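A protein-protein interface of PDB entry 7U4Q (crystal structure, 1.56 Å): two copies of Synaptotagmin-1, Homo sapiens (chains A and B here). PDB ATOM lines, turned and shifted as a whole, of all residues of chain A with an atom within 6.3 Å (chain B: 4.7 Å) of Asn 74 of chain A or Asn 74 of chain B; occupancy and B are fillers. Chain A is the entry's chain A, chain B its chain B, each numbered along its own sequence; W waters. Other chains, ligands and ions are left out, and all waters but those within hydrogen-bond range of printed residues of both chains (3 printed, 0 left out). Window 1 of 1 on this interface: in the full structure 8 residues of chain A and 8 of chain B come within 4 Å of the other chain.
The side-chain amide nitrogen (ND2) of Asn 74 of chain B is in hydrogen-bond range of the side-chain amide oxygen (OD1) of Asn 74 of chain A, at 2.7 Å.
The backbone carbonyl oxygen (O) of Glu 75 of chain B is in hydrogen-bond range of the side-chain amide nitrogen (ND2) of Asn 74 of chain A, at 3.2 Å.
The backbone carbonyl oxygen of Ser 15 of chain A is in hydrogen-bond range of the backbone NH of Gly 28 of chain A (2.8 Å).
The backbone NH of Asn 74 of chain A sits at hydrogen-bond distance from the backbone carbonyl oxygen of Ile 29 of chain A, 3.3 Å away.
O of Glu 75 of chain A is in hydrogen-bond range of N of Ile 29 of chain A.
The side-chain carboxylate (OE2) of Glu 75 of chain A lies within salt-bridge range of the side-chain amino group (NZ) of Lys 63 of chain A (3.6 Å).
The backbone carbonyl oxygen of Ile 29 of chain B sits at hydrogen-bond distance from the backbone NH of Asn 74 of chain B, 3.3 Å away.
N of Asn 74 of chain B is in hydrogen-bond range of O of Ile 30 of chain B (2.9 Å).
Among the printed residues, merely in contact across the chains: Gly 28 of chain A with Asn 74 of chain B, Ile 30 of chain A with Val 72 of chain B, Ile 30 of chain A with Asn 74 of chain B, Val 72 of chain A with Ile 30 of chain B, Asn 74 of chain A with Gly 28 of chain B, Asn 74 of chain A with Ile 30 of chain B and Glu 75 of chain A with Asn 74 of chain B.
Of the printed residues of chain B, Asn 74 of chain A touches Gly 28 (3.6 Å), Ile 30 (3.7 Å), Asn 74 (2.7 Å) and Glu 75 (3.2 Å).
Asn 74 of chain B touches just these residues of chain A: Gly 28 (3.5 Å), Ile 30 (3.8 Å), Asn 74 (2.7 Å) and Glu 75 (3.6 Å).
Of the printed residues of chain A, Gly 28 of chain B touches Asn 74 (3.6 Å).
Of the printed residues of chain A, Ile 30 of chain B touches Val 72 (3.8 Å) and Asn 74 (3.7 Å).
Gln 76 of chain B touches none of the printed residues of chain A.
The nearest residue of chain B that does not touch Asn 74 of chain A is Ile 29 of chain B (4.04 Å).
Printed residues of chain B that touch a printed residue of chain A: Gly 28, Ile 30, Val 72, Asn 74 and Glu 75.
Of the 13 printed residues of chain A, 5 touch a printed residue of chain B.
Hydrophobic or aromatic side chains of chain A within 4 Å of the printed part of chain B: Ile 30 and Val 72.
Along chain A the printed residues that touch a printed residue of chain B span positions 28 to 75.
Among the printed residues, no Asp or Glu carboxylate lies within 4 Å of a Lys or Arg side-chain nitrogen of the other chain.
Ile 30 of chain A touches Val 72 of chain B, and with the chains exchanged Val 72 of chain A touches Ile 30 of chain B.
Ile 30 of chain A touches Asn 74 of chain B, and with the chains exchanged Asn 74 of chain A touches Ile 30 of chain B.
Asn 74 of chain A touches its own counterpart, Asn 74 of chain B.
Asn 74 of chain A touches Glu 75 of chain B, and with the chains exchanged Glu 75 of chain A touches Asn 74 of chain B.
Of the 9 pairs that touch across the chains among the printed residues, 9 have their exchanged pair printed and touching as well.
Water W2 bridges the side-chain hydroxyl (OG) of Ser 15 of chain A (2.5 Å) and the side-chain amide oxygen (OD1) of Asn 74 of chain B (3.0 Å).
Water W3 bridges the backbone carbonyl oxygen of Asn 74 of chain A (2.8 Å) and the side-chain amide nitrogen of Gln 76 of chain B (3.3 Å).
Water W1 bridges O of Asn 74 of chain B and O of Asn 74 of chain A.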
ATOM      1  N   SER A  15     -33.321 -26.474  -2.908  1.00  0.00           N
ATOM      2  CA  SER A  15     -33.657 -26.795  -1.522  1.00  0.00           C
ATOM      3  C   SER A  15     -33.814 -25.493  -0.753  1.00  0.00           C
ATOM      4  O   SER A  15     -33.198 -24.487  -1.111  1.00  0.00           O
ATOM      5  CB  SER A  15     -32.556 -27.630  -0.893  1.00  0.00           C
ATOM      6  OG  SER A  15     -31.379 -26.848  -0.698  1.00  0.00           O
ATOM      7  N   VAL A  27     -30.915 -20.935   0.248  1.00  0.00           N
ATOM      8  CA  VAL A  27     -31.479 -21.448  -0.986  1.00  0.00           C
ATOM      9  C   VAL A  27     -30.394 -22.234  -1.711  1.00  0.00           C
ATOM     10  O   VAL A  27     -29.400 -21.654  -2.149  1.00  0.00           O
ATOM     11  CB  VAL A  27     -31.970 -20.318  -1.898  1.00  0.00           C
ATOM     12  CG1 VAL A  27     -32.536 -20.867  -3.204  1.00  0.00           C
ATOM     13  CG2 VAL A  27     -32.984 -19.451  -1.183  1.00  0.00           C
ATOM     14  N   GLY A  28     -30.604 -23.551  -1.826  1.00  0.00           N
ATOM     15  CA  GLY A  28     -29.723 -24.434  -2.572  1.00  0.00           C
ATOM     16  C   GLY A  28     -30.204 -24.495  -4.011  1.00  0.00           C
ATOM     17  O   GLY A  28     -31.364 -24.768  -4.267  1.00  0.00           O
ATOM     18  N   ILE A  29     -29.323 -24.151  -4.960  1.00  0.00           N
ATOM     19  CA  ILE A  29     -29.581 -24.343  -6.397  1.00  0.00           C
ATOM     20  C   ILE A  29     -28.691 -25.489  -6.857  1.00  0.00           C
ATOM     21  O   ILE A  29     -27.473 -25.342  -7.029  1.00  0.00           O
ATOM     22  CB  ILE A  29     -29.300 -23.054  -7.210  1.00  0.00           C
ATOM     23  CG1 ILE A  29     -30.109 -21.868  -6.663  1.00  0.00           C
ATOM     24  CG2 ILE A  29     -29.612 -23.280  -8.697  1.00  0.00           C
ATOM     25  CD1 ILE A  29     -31.617 -22.037  -6.712  1.00  0.00           C
ATOM     26  N   ILE A  30     -29.292 -26.676  -7.007  1.00  0.00           N
ATOM     27  CA  ILE A  30     -28.523 -27.883  -7.099  1.00  0.00           C
ATOM     28  C   ILE A  30     -28.163 -28.174  -8.572  1.00  0.00           C
ATOM     29  O   ILE A  30     -26.990 -28.298  -8.916  1.00  0.00           O
ATOM     30  CB  ILE A  30     -29.258 -29.079  -6.459  1.00  0.00           C
ATOM     31  CG1 ILE A  30     -29.575 -28.750  -4.984  1.00  0.00           C
ATOM     32  CG2 ILE A  30     -28.403 -30.317  -6.553  1.00  0.00           C
ATOM     33  CD1 ILE A  30     -30.768 -29.516  -4.442  1.00  0.00           C
ATOM     34  N   GLN A  31     -29.188 -28.318  -9.409  1.00  0.00           N
ATOM     35  CA  GLN A  31     -29.005 -28.670 -10.823  1.00  0.00           C
ATOM     36  C   GLN A  31     -30.266 -28.379 -11.590  1.00  0.00           C
ATOM     37  O   GLN A  31     -31.344 -28.173 -11.007  1.00  0.00           O
ATOM     38  CB  GLN A  31     -28.627 -30.148 -10.956  1.00  0.00           C
ATOM     39  CG  GLN A  31     -29.678 -31.089 -10.411  1.00  0.00           C
ATOM     40  CD  GLN A  31     -29.312 -32.552 -10.558  1.00  0.00           C
ATOM     41  OE1 GLN A  31     -28.815 -32.982 -11.580  1.00  0.00           O
ATOM     42  NE2 GLN A  31     -29.584 -33.326  -9.531  1.00  0.00           N
ATOM     43  N   LYS A  63     -23.008 -19.297 -11.312  1.00  0.00           N
ATOM     44  CA  LYS A  63     -22.070 -19.387 -12.420  1.00  0.00           C
ATOM     45  C   LYS A  63     -22.820 -19.793 -13.680  1.00  0.00           C
ATOM     46  O   LYS A  63     -23.865 -20.490 -13.627  1.00  0.00           O
ATOM     47  CB  LYS A  63     -20.986 -20.412 -12.127  1.00  0.00           C
ATOM     48  CG  LYS A  63     -20.076 -20.057 -10.956  1.00  0.00           C
ATOM     49  CD  LYS A  63     -18.806 -20.918 -10.935  1.00  0.00           C
ATOM     50  CE  LYS A  63     -19.077 -22.327 -10.444  1.00  0.00           C
ATOM     51  NZ  LYS A  63     -19.626 -22.421  -9.048  1.00  0.00           N
ATOM     52  N   HIS A  65     -22.870 -22.115 -16.772  1.00  0.00           N
ATOM     53  CA  HIS A  65     -22.378 -23.422 -17.176  1.00  0.00           C
ATOM     54  C   HIS A  65     -22.463 -23.499 -18.697  1.00  0.00           C
ATOM     55  O   HIS A  65     -23.506 -23.319 -19.271  1.00  0.00           O
ATOM     56  CB  HIS A  65     -23.150 -24.506 -16.488  1.00  0.00           C
ATOM     57  CG  HIS A  65     -22.742 -24.699 -15.066  1.00  0.00           C
ATOM     58  ND1 HIS A  65     -22.114 -25.844 -14.620  1.00  0.00           N
ATOM     59  CD2 HIS A  65     -22.798 -23.860 -13.994  1.00  0.00           C
ATOM     60  CE1 HIS A  65     -21.793 -25.698 -13.344  1.00  0.00           C
ATOM     61  NE2 HIS A  65     -22.215 -24.516 -12.939  1.00  0.00           N
ATOM     62  N   VAL A  72     -25.056 -28.808 -13.441  1.00  0.00           N
ATOM     63  CA  VAL A  72     -24.984 -29.115 -12.022  1.00  0.00           C
ATOM     64  C   VAL A  72     -24.349 -27.910 -11.354  1.00  0.00           C
ATOM     65  O   VAL A  72     -23.138 -27.756 -11.368  1.00  0.00           O
ATOM     66  CB  VAL A  72     -24.215 -30.403 -11.745  1.00  0.00           C
ATOM     67  CG1 VAL A  72     -24.198 -30.676 -10.238  1.00  0.00           C
ATOM     68  CG2 VAL A  72     -24.847 -31.563 -12.522  1.00  0.00           C
ATOM     69  N   PHE A  73     -25.200 -27.024 -10.832  1.00  0.00           N
ATOM     70  CA  PHE A  73     -24.753 -25.774 -10.230  1.00  0.00           C
ATOM     71  C   PHE A  73     -24.046 -25.970  -8.903  1.00  0.00           C
ATOM     72  O   PHE A  73     -23.002 -25.378  -8.640  1.00  0.00           O
ATOM     73  CB  PHE A  73     -25.908 -24.806 -10.095  1.00  0.00           C
ATOM     74  CG  PHE A  73     -26.548 -24.433 -11.399  1.00  0.00           C
ATOM     75  CD1 PHE A  73     -25.877 -23.609 -12.272  1.00  0.00           C
ATOM     76  CD2 PHE A  73     -27.824 -24.912 -11.760  1.00  0.00           C
ATOM     77  CE1 PHE A  73     -26.435 -23.266 -13.496  1.00  0.00           C
ATOM     78  CE2 PHE A  73     -28.388 -24.543 -12.961  1.00  0.00           C
ATOM     79  CZ  PHE A  73     -27.679 -23.715 -13.832  1.00  0.00           C
ATOM     80  N   ASN A  74     -24.634 -26.773  -8.023  1.00  0.00           N
ATOM     81  CA  ASN A  74     -24.094 -26.999  -6.713  1.00  0.00           C
ATOM     82  C   ASN A  74     -23.765 -25.699  -5.969  1.00  0.00           C
ATOM     83  O   ASN A  74     -22.659 -25.558  -5.427  1.00  0.00           O
ATOM     84  CB  ASN A  74     -22.867 -27.896  -6.752  1.00  0.00           C
ATOM     85  CG  ASN A  74     -22.464 -28.380  -5.356  1.00  0.00           C
ATOM     86  OD1 ASN A  74     -23.306 -28.542  -4.493  1.00  0.00           O
ATOM     87  ND2 ASN A  74     -21.225 -28.613  -5.144  1.00  0.00           N
ATOM     88  N   GLU A  75     -24.727 -24.771  -5.946  1.00  0.00           N
ATOM     89  CA  GLU A  75     -24.548 -23.506  -5.239  1.00  0.00           C
ATOM     90  C   GLU A  75     -25.548 -23.317  -4.118  1.00  0.00           C
ATOM     91  O   GLU A  75     -26.596 -23.958  -4.087  1.00  0.00           O
ATOM     92  CB  GLU A  75     -24.589 -22.336  -6.207  1.00  0.00           C
ATOM     93  CG  GLU A  75     -23.402 -22.374  -7.149  1.00  0.00           C
ATOM     94  CD  GLU A  75     -23.242 -21.108  -7.949  1.00  0.00           C
ATOM     95  OE1 GLU A  75     -23.343 -19.999  -7.367  1.00  0.00           O
ATOM     96  OE2 GLU A  75     -22.995 -21.219  -9.170  1.00  0.00           O
ATOM     97  N   GLN A  76     -25.177 -22.466  -3.159  1.00  0.00           N
ATOM     98  CA  GLN A  76     -26.043 -22.068  -2.075  1.00  0.00           C
ATOM     99  C   GLN A  76     -26.002 -20.555  -1.917  1.00  0.00           C
ATOM    100  O   GLN A  76     -24.911 -19.977  -1.870  1.00  0.00           O
ATOM    101  CB  GLN A  76     -25.634 -22.754  -0.779  1.00  0.00           C
ATOM    102  CG  GLN A  76     -26.614 -22.448   0.360  1.00  0.00           C
ATOM    103  CD  GLN A  76     -26.066 -22.803   1.756  1.00  0.00           C
ATOM    104  OE1 GLN A  76     -25.344 -22.009   2.399  1.00  0.00           O
ATOM    105  NE2 GLN A  76     -26.436 -23.984   2.247  1.00  0.00           N
ATOM    106  N   GLY B  28     -16.468 -29.742  -4.575  1.00  0.00           N
ATOM    107  CA  GLY B  28     -17.908 -29.830  -4.532  1.00  0.00           C
ATOM    108  C   GLY B  28     -18.300 -31.253  -4.200  1.00  0.00           C
ATOM    109  O   GLY B  28     -17.847 -32.198  -4.859  1.00  0.00           O
ATOM    110  N   ILE B  29     -19.125 -31.429  -3.153  1.00  0.00           N
ATOM    111  CA  ILE B  29     -19.729 -32.737  -2.831  1.00  0.00           C
ATOM    112  C   ILE B  29     -21.205 -32.609  -3.125  1.00  0.00           C
ATOM    113  O   ILE B  29     -21.968 -31.973  -2.383  1.00  0.00           O
ATOM    114  CB  ILE B  29     -19.458 -33.162  -1.379  1.00  0.00           C
ATOM    115  CG1 ILE B  29     -17.957 -33.155  -1.052  1.00  0.00           C
ATOM    116  CG2 ILE B  29     -20.091 -34.516  -1.072  1.00  0.00           C
ATOM    117  CD1 ILE B  29     -17.140 -34.144  -1.860  1.00  0.00           C
ATOM    118  N   ILE B  30     -21.632 -33.180  -4.267  1.00  0.00           N
ATOM    119  CA  ILE B  30     -22.929 -32.860  -4.795  1.00  0.00           C
ATOM    120  C   ILE B  30     -23.989 -33.824  -4.229  1.00  0.00           C
ATOM    121  O   ILE B  30     -24.979 -33.385  -3.654  1.00  0.00           O
ATOM    122  CB  ILE B  30     -22.934 -32.863  -6.331  1.00  0.00           C
ATOM    123  CG1 ILE B  30     -21.887 -31.842  -6.857  1.00  0.00           C
ATOM    124  CG2 ILE B  30     -24.328 -32.518  -6.855  1.00  0.00           C
ATOM    125  CD1 ILE B  30     -21.334 -32.205  -8.210  1.00  0.00           C
ATOM    126  N   VAL B  72     -28.590 -35.853  -1.288  1.00  0.00           N
ATOM    127  CA  VAL B  72     -28.172 -34.701  -2.073  1.00  0.00           C
ATOM    128  C   VAL B  72     -27.536 -33.732  -1.078  1.00  0.00           C
ATOM    129  O   VAL B  72     -28.235 -33.030  -0.355  1.00  0.00           O
ATOM    130  CB  VAL B  72     -29.339 -34.056  -2.819  1.00  0.00           C
ATOM    131  CG1 VAL B  72     -28.833 -32.845  -3.603  1.00  0.00           C
ATOM    132  CG2 VAL B  72     -29.998 -35.091  -3.714  1.00  0.00           C
ATOM    133  N   PHE B  73     -26.203 -33.746  -1.035  1.00  0.00           N
ATOM    134  CA  PHE B  73     -25.442 -32.927  -0.101  1.00  0.00           C
ATOM    135  C   PHE B  73     -25.427 -31.456  -0.482  1.00  0.00           C
ATOM    136  O   PHE B  73     -25.609 -30.573   0.353  1.00  0.00           O
ATOM    137  CB  PHE B  73     -24.014 -33.469   0.017  1.00  0.00           C
ATOM    138  CG  PHE B  73     -23.951 -34.877   0.537  1.00  0.00           C
ATOM    139  CD1 PHE B  73     -24.279 -35.152   1.864  1.00  0.00           C
ATOM    140  CD2 PHE B  73     -23.639 -35.949  -0.304  1.00  0.00           C
ATOM    141  CE1 PHE B  73     -24.234 -36.442   2.345  1.00  0.00           C
ATOM    142  CE2 PHE B  73     -23.610 -37.236   0.183  1.00  0.00           C
ATOM    143  CZ  PHE B  73     -23.903 -37.481   1.505  1.00  0.00           C
ATOM    144  N   ASN B  74     -25.152 -31.165  -1.756  1.00  0.00           N
ATOM    145  CA  ASN B  74     -25.067 -29.787  -2.233  1.00  0.00           C
ATOM    146  C   ASN B  74     -24.127 -28.927  -1.374  1.00  0.00           C
ATOM    147  O   ASN B  74     -24.512 -27.832  -0.934  1.00  0.00           O
ATOM    148  CB  ASN B  74     -26.484 -29.221  -2.250  1.00  0.00           C
ATOM    149  CG  ASN B  74     -26.582 -27.824  -2.802  1.00  0.00           C
ATOM    150  OD1 ASN B  74     -27.407 -27.029  -2.401  1.00  0.00           O
ATOM    151  ND2 ASN B  74     -25.759 -27.552  -3.772  1.00  0.00           N
ATOM    152  N   GLU B  75     -22.927 -29.441  -1.114  1.00  0.00           N
ATOM    153  CA  GLU B  75     -21.926 -28.713  -0.334  1.00  0.00           C
ATOM    154  C   GLU B  75     -20.657 -28.382  -1.139  1.00  0.00           C
ATOM    155  O   GLU B  75     -20.336 -29.013  -2.147  1.00  0.00           O
ATOM    156  CB  GLU B  75     -21.593 -29.496   0.918  1.00  0.00           C
ATOM    157  CG  GLU B  75     -22.792 -29.480   1.850  1.00  0.00           C
ATOM    158  CD  GLU B  75     -22.494 -29.832   3.271  1.00  0.00           C
ATOM    159  OE1 GLU B  75     -21.474 -29.367   3.832  1.00  0.00           O
ATOM    160  OE2 GLU B  75     -23.310 -30.587   3.824  1.00  0.00           O
ATOM    161  N   GLN B  76     -19.929 -27.377  -0.652  1.00  0.00           N
ATOM    162  CA  GLN B  76     -18.671 -26.950  -1.234  1.00  0.00           C
ATOM    163  C   GLN B  76     -17.680 -26.705  -0.112  1.00  0.00           C
ATOM    164  O   GLN B  76     -18.026 -26.026   0.869  1.00  0.00           O
ATOM    165  CB  GLN B  76     -18.887 -25.619  -1.948  1.00  0.00           C
ATOM    166  CG  GLN B  76     -18.769 -25.682  -3.448  1.00  0.00           C
ATOM    167  CD  GLN B  76     -17.331 -25.702  -3.990  1.00  0.00           C
ATOM    168  OE1 GLN B  76     -16.407 -25.197  -3.309  1.00  0.00           O
ATOM    169  NE2 GLN B  76     -17.128 -26.255  -5.216  1.00  0.00           N
HETATM  170  O   HOH W   1     -23.118 -25.621  -2.403  1.00  0.00           O
HETATM  171  O   HOH W   2     -29.370 -28.269  -0.500  1.00  0.00           O
HETATM  172  O   HOH W   3     -20.052 -24.875  -5.986  1.00  0.00           O
